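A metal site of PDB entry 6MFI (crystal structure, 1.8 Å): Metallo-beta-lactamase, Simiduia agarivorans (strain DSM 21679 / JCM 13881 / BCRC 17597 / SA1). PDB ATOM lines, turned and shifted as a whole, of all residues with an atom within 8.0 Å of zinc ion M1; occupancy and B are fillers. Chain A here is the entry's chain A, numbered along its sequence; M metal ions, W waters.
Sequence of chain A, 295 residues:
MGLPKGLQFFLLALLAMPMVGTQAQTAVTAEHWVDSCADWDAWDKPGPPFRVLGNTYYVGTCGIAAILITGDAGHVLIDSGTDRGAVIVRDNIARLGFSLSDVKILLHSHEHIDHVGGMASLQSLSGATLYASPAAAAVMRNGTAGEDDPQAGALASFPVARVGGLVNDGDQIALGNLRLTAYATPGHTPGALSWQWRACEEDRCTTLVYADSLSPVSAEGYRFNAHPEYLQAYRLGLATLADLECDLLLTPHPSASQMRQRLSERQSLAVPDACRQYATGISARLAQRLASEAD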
ATOM      1  N   TRP A  40      30.193 -34.231  -6.896  1.00  0.00           N
ATOM      2  CA  TRP A  40      31.005 -33.186  -6.254  1.00  0.00           C
ATOM      3  C   TRP A  40      31.256 -32.028  -7.219  1.00  0.00           C
ATOM      4  O   TRP A  40      32.385 -31.586  -7.414  1.00  0.00           O
ATOM      5  CB  TRP A  40      32.318 -33.768  -5.732  1.00  0.00           C
ATOM      6  CG  TRP A  40      32.139 -34.846  -4.714  1.00  0.00           C
ATOM      7  CD1 TRP A  40      32.472 -36.171  -4.848  1.00  0.00           C
ATOM      8  CD2 TRP A  40      31.602 -34.710  -3.394  1.00  0.00           C
ATOM      9  NE1 TRP A  40      32.164 -36.849  -3.700  1.00  0.00           N
ATOM     10  CE2 TRP A  40      31.635 -35.981  -2.787  1.00  0.00           C
ATOM     11  CE3 TRP A  40      31.083 -33.623  -2.664  1.00  0.00           C
ATOM     12  CZ2 TRP A  40      31.171 -36.198  -1.494  1.00  0.00           C
ATOM     13  CZ3 TRP A  40      30.628 -33.851  -1.382  1.00  0.00           C
ATOM     14  CH2 TRP A  40      30.670 -35.126  -0.810  1.00  0.00           C
ATOM     15  N   TRP A  43      30.029 -25.487  -6.632  1.00  0.00           N
ATOM     16  CA  TRP A  43      28.933 -25.015  -5.792  1.00  0.00           C
ATOM     17  C   TRP A  43      27.970 -24.120  -6.560  1.00  0.00           C
ATOM     18  O   TRP A  43      26.758 -24.183  -6.353  1.00  0.00           O
ATOM     19  CB  TRP A  43      29.486 -24.272  -4.578  1.00  0.00           C
ATOM     20  CG  TRP A  43      30.203 -25.145  -3.591  1.00  0.00           C
ATOM     21  CD1 TRP A  43      30.163 -26.516  -3.532  1.00  0.00           C
ATOM     22  CD2 TRP A  43      31.057 -24.724  -2.533  1.00  0.00           C
ATOM     23  NE1 TRP A  43      30.944 -26.965  -2.496  1.00  0.00           N
ATOM     24  CE2 TRP A  43      31.505 -25.881  -1.868  1.00  0.00           C
ATOM     25  CE3 TRP A  43      31.501 -23.482  -2.082  1.00  0.00           C
ATOM     26  CZ2 TRP A  43      32.364 -25.827  -0.767  1.00  0.00           C
ATOM     27  CZ3 TRP A  43      32.357 -23.431  -0.990  1.00  0.00           C
ATOM     28  CH2 TRP A  43      32.786 -24.597  -0.349  1.00  0.00           C
ATOM     29  N   GLY A  63      26.137 -28.611  -7.197  1.00  0.00           N
ATOM     30  CA  GLY A  63      27.041 -28.883  -6.099  1.00  0.00           C
ATOM     31  C   GLY A  63      26.441 -28.596  -4.733  1.00  0.00           C
ATOM     32  O   GLY A  63      26.923 -29.136  -3.724  1.00  0.00           O
ATOM     33  N   ILE A  64      25.405 -27.764  -4.675  1.00  0.00           N
ATOM     34  CA  ILE A  64      24.767 -27.382  -3.420  1.00  0.00           C
ATOM     35  C   ILE A  64      23.273 -27.648  -3.531  1.00  0.00           C
ATOM     36  O   ILE A  64      22.641 -27.268  -4.522  1.00  0.00           O
ATOM     37  CB  ILE A  64      25.026 -25.893  -3.083  1.00  0.00           C
ATOM     38  CG1 ILE A  64      26.526 -25.657  -2.857  1.00  0.00           C
ATOM     39  CG2 ILE A  64      24.230 -25.484  -1.859  1.00  0.00           C
ATOM     40  CD1 ILE A  64      27.105 -26.451  -1.714  1.00  0.00           C
ATOM     41  N   SER A 109      20.383 -25.846   6.692  1.00  0.00           N
ATOM     42  CA  SER A 109      21.107 -27.006   7.199  1.00  0.00           C
ATOM     43  C   SER A 109      22.121 -26.537   8.245  1.00  0.00           C
ATOM     44  O   SER A 109      21.911 -26.730   9.447  1.00  0.00           O
ATOM     45  CB  SER A 109      21.810 -27.747   6.063  1.00  0.00           C
ATOM     46  OG  SER A 109      22.658 -26.889   5.327  1.00  0.00           O
ATOM     47  N   HIS A 110      23.218 -25.932   7.788  1.00  0.00           N
ATOM     48  CA  HIS A 110      24.183 -25.314   8.690  1.00  0.00           C
ATOM     49  C   HIS A 110      24.646 -23.990   8.098  1.00  0.00           C
ATOM     50  O   HIS A 110      24.489 -23.730   6.904  1.00  0.00           O
ATOM     51  CB  HIS A 110      25.363 -26.242   8.991  1.00  0.00           C
ATOM     52  CG  HIS A 110      26.190 -26.587   7.793  1.00  0.00           C
ATOM     53  ND1 HIS A 110      26.019 -27.766   7.092  1.00  0.00           N
ATOM     54  CD2 HIS A 110      27.210 -25.935   7.186  1.00  0.00           C
ATOM     55  CE1 HIS A 110      26.882 -27.813   6.095  1.00  0.00           C
ATOM     56  NE2 HIS A 110      27.619 -26.721   6.139  1.00  0.00           N
ATOM     57  N   HIS A 112      27.116 -22.297   6.938  1.00  0.00           N
ATOM     58  CA  HIS A 112      28.285 -22.037   6.114  1.00  0.00           C
ATOM     59  C   HIS A 112      27.870 -21.290   4.842  1.00  0.00           C
ATOM     60  O   HIS A 112      26.727 -21.385   4.392  1.00  0.00           O
ATOM     61  CB  HIS A 112      29.006 -23.327   5.764  1.00  0.00           C
ATOM     62  CG  HIS A 112      29.961 -23.792   6.822  1.00  0.00           C
ATOM     63  ND1 HIS A 112      30.743 -24.925   6.670  1.00  0.00           N
ATOM     64  CD2 HIS A 112      30.251 -23.283   8.035  1.00  0.00           C
ATOM     65  CE1 HIS A 112      31.482 -25.082   7.760  1.00  0.00           C
ATOM     66  NE2 HIS A 112      31.209 -24.102   8.600  1.00  0.00           N
ATOM     67  N   ILE A 113      28.829 -20.549   4.285  1.00  0.00           N
ATOM     68  CA  ILE A 113      28.515 -19.630   3.183  1.00  0.00           C
ATOM     69  C   ILE A 113      28.022 -20.381   1.951  1.00  0.00           C
ATOM     70  O   ILE A 113      27.229 -19.844   1.179  1.00  0.00           O
ATOM     71  CB  ILE A 113      29.758 -18.765   2.857  1.00  0.00           C
ATOM     72  CG1 ILE A 113      29.421 -17.732   1.774  1.00  0.00           C
ATOM     73  CG2 ILE A 113      30.932 -19.632   2.435  1.00  0.00           C
ATOM     74  CD1 ILE A 113      30.597 -16.881   1.354  1.00  0.00           C
ATOM     75  N   ASP A 114      28.461 -21.628   1.761  1.00  0.00           N
ATOM     76  CA  ASP A 114      28.038 -22.364   0.577  1.00  0.00           C
ATOM     77  C   ASP A 114      26.599 -22.860   0.673  1.00  0.00           C
ATOM     78  O   ASP A 114      26.081 -23.402  -0.301  1.00  0.00           O
ATOM     79  CB  ASP A 114      28.974 -23.551   0.323  1.00  0.00           C
ATOM     80  CG  ASP A 114      29.128 -24.449   1.528  1.00  0.00           C
ATOM     81  OD1 ASP A 114      29.281 -23.917   2.651  1.00  0.00           O
ATOM     82  OD2 ASP A 114      29.096 -25.682   1.362  1.00  0.00           O
ATOM     83  N   HIS A 115      25.945 -22.692   1.818  1.00  0.00           N
ATOM     84  CA  HIS A 115      24.563 -23.136   2.000  1.00  0.00           C
ATOM     85  C   HIS A 115      23.594 -22.020   2.361  1.00  0.00           C
ATOM     86  O   HIS A 115      22.415 -22.115   2.021  1.00  0.00           O
ATOM     87  CB  HIS A 115      24.485 -24.219   3.083  1.00  0.00           C
ATOM     88  CG  HIS A 115      25.355 -25.408   2.797  1.00  0.00           C
ATOM     89  ND1 HIS A 115      25.160 -26.236   1.715  1.00  0.00           N
ATOM     90  CD2 HIS A 115      26.436 -25.905   3.462  1.00  0.00           C
ATOM     91  CE1 HIS A 115      26.070 -27.192   1.723  1.00  0.00           C
ATOM     92  NE2 HIS A 115      26.853 -27.010   2.771  1.00  0.00           N
ATOM     93  N   GLN A 151      35.321 -24.332  10.917  1.00  0.00           N
ATOM     94  CA  GLN A 151      35.927 -23.732   9.744  1.00  0.00           C
ATOM     95  C   GLN A 151      36.003 -22.207   9.849  1.00  0.00           C
ATOM     96  O   GLN A 151      35.924 -21.506   8.835  1.00  0.00           O
ATOM     97  CB  GLN A 151      35.167 -24.136   8.486  1.00  0.00           C
ATOM     98  CG  GLN A 151      36.014 -24.225   7.233  1.00  0.00           C
ATOM     99  CD  GLN A 151      35.234 -24.708   6.026  1.00  0.00           C
ATOM    100  OE1 GLN A 151      34.397 -25.599   6.124  1.00  0.00           O
ATOM    101  NE2 GLN A 151      35.510 -24.102   4.875  1.00  0.00           N
ATOM    102  N   HIS A 188      29.730 -30.305  12.536  1.00  0.00           N
ATOM    103  CA  HIS A 188      30.234 -29.546  11.397  1.00  0.00           C
ATOM    104  C   HIS A 188      30.161 -28.047  11.668  1.00  0.00           C
ATOM    105  O   HIS A 188      31.099 -27.311  11.338  1.00  0.00           O
ATOM    106  CB  HIS A 188      29.434 -29.907  10.141  1.00  0.00           C
ATOM    107  CG  HIS A 188      29.950 -29.271   8.891  1.00  0.00           C
ATOM    108  ND1 HIS A 188      31.040 -29.759   8.199  1.00  0.00           N
ATOM    109  CD2 HIS A 188      29.531 -28.183   8.213  1.00  0.00           C
ATOM    110  CE1 HIS A 188      31.271 -29.000   7.141  1.00  0.00           C
ATOM    111  NE2 HIS A 188      30.368 -28.032   7.128  1.00  0.00           N
ATOM    112  N   THR A 189      29.070 -27.588  12.260  1.00  0.00           N
ATOM    113  CA  THR A 189      28.904 -26.238  12.755  1.00  0.00           C
ATOM    114  C   THR A 189      28.211 -26.312  14.109  1.00  0.00           C
ATOM    115  O   THR A 189      27.578 -27.332  14.425  1.00  0.00           O
ATOM    116  CB  THR A 189      28.060 -25.370  11.802  1.00  0.00           C
ATOM    117  OG1 THR A 189      26.708 -25.842  11.797  1.00  0.00           O
ATOM    118  CG2 THR A 189      28.617 -25.392  10.389  1.00  0.00           C
ATOM    119  N   ASP A 212      22.255 -32.993   7.817  1.00  0.00           N
ATOM    120  CA  ASP A 212      23.330 -32.039   7.632  1.00  0.00           C
ATOM    121  C   ASP A 212      24.609 -32.742   7.164  1.00  0.00           C
ATOM    122  O   ASP A 212      24.738 -33.966   7.223  1.00  0.00           O
ATOM    123  CB  ASP A 212      23.576 -31.273   8.932  1.00  0.00           C
ATOM    124  CG  ASP A 212      24.555 -30.120   8.758  1.00  0.00           C
ATOM    125  OD1 ASP A 212      24.192 -29.130   8.099  1.00  0.00           O
ATOM    126  OD2 ASP A 212      25.685 -30.212   9.285  1.00  0.00           O
ATOM    127  N   SER A 213      25.565 -31.935   6.688  1.00  0.00           N
ATOM    128  CA  SER A 213      26.834 -32.474   6.211  1.00  0.00           C
ATOM    129  C   SER A 213      27.513 -33.308   7.287  1.00  0.00           C
ATOM    130  O   SER A 213      28.011 -34.410   7.005  1.00  0.00           O
ATOM    131  CB  SER A 213      27.737 -31.332   5.750  1.00  0.00           C
ATOM    132  OG  SER A 213      27.106 -30.567   4.741  1.00  0.00           O
ATOM    133  N   SER A 215      30.224 -33.436   8.491  1.00  0.00           N
ATOM    134  CA  SER A 215      31.595 -33.859   8.220  1.00  0.00           C
ATOM    135  C   SER A 215      32.550 -33.271   9.253  1.00  0.00           C
ATOM    136  O   SER A 215      32.463 -32.081   9.570  1.00  0.00           O
ATOM    137  CB  SER A 215      32.013 -33.432   6.820  1.00  0.00           C
ATOM    138  OG  SER A 215      31.759 -32.056   6.619  1.00  0.00           O
ATOM    139  N   VAL A 217      35.252 -31.870   9.184  1.00  0.00           N
ATOM    140  CA  VAL A 217      36.178 -31.007   8.485  1.00  0.00           C
ATOM    141  C   VAL A 217      36.226 -29.674   9.219  1.00  0.00           C
ATOM    142  O   VAL A 217      35.272 -29.278   9.912  1.00  0.00           O
ATOM    143  CB  VAL A 217      35.790 -30.818   6.996  1.00  0.00           C
ATOM    144  CG1 VAL A 217      34.593 -29.891   6.875  1.00  0.00           C
ATOM    145  CG2 VAL A 217      36.972 -30.312   6.178  1.00  0.00           C
ATOM    146  N   PRO A 252      22.890 -31.571   1.955  1.00  0.00           N
ATOM    147  CA  PRO A 252      23.219 -30.275   1.340  1.00  0.00           C
ATOM    148  C   PRO A 252      24.272 -30.376   0.250  1.00  0.00           C
ATOM    149  O   PRO A 252      24.208 -29.635  -0.736  1.00  0.00           O
ATOM    150  CB  PRO A 252      23.717 -29.445   2.537  1.00  0.00           C
ATOM    151  CG  PRO A 252      23.091 -30.090   3.719  1.00  0.00           C
ATOM    152  CD  PRO A 252      23.045 -31.552   3.412  1.00  0.00           C
ATOM    153  N   HIS A 253      25.241 -31.279   0.409  1.00  0.00           N
ATOM    154  CA  HIS A 253      26.091 -31.674  -0.696  1.00  0.00           C
ATOM    155  C   HIS A 253      25.522 -32.959  -1.267  1.00  0.00           C
ATOM    156  O   HIS A 253      25.572 -34.004  -0.597  1.00  0.00           O
ATOM    157  CB  HIS A 253      27.529 -31.881  -0.241  1.00  0.00           C
ATOM    158  CG  HIS A 253      28.183 -30.637   0.279  1.00  0.00           C
ATOM    159  ND1 HIS A 253      28.774 -29.704  -0.554  1.00  0.00           N
ATOM    160  CD2 HIS A 253      28.346 -30.171   1.536  1.00  0.00           C
ATOM    161  CE1 HIS A 253      29.260 -28.725   0.171  1.00  0.00           C
ATOM    162  NE2 HIS A 253      29.012 -28.976   1.445  1.00  0.00           N
HETATM  163 ZN    ZN M   1      29.051 -27.254   2.643  1.00  0.00          ZN
HETATM  164 ZN    ZN M   2      29.798 -26.534   5.878  1.00  0.00          ZN
HETATM  165  O   HOH W   1      30.324 -26.520   3.976  1.00  0.00           O
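A ring nitrogen (ND1) of His 110 is in hydrogen-bond range of the side-chain carboxylate of Asp 212 (2.5 Å).
His 110 touches zinc ion M1 (NE2 to ZN, 3.8 Å). Of the 19 residues printed, 4 come within 4 Å of zinc ion M1.
Zinc ion M1 is bound by water W1 (2.0 Å), OD2 of Asp 114 (2.0 Å), NE2 of His 253 (2.1 Å) and NE2 of His 115 (2.2 Å).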
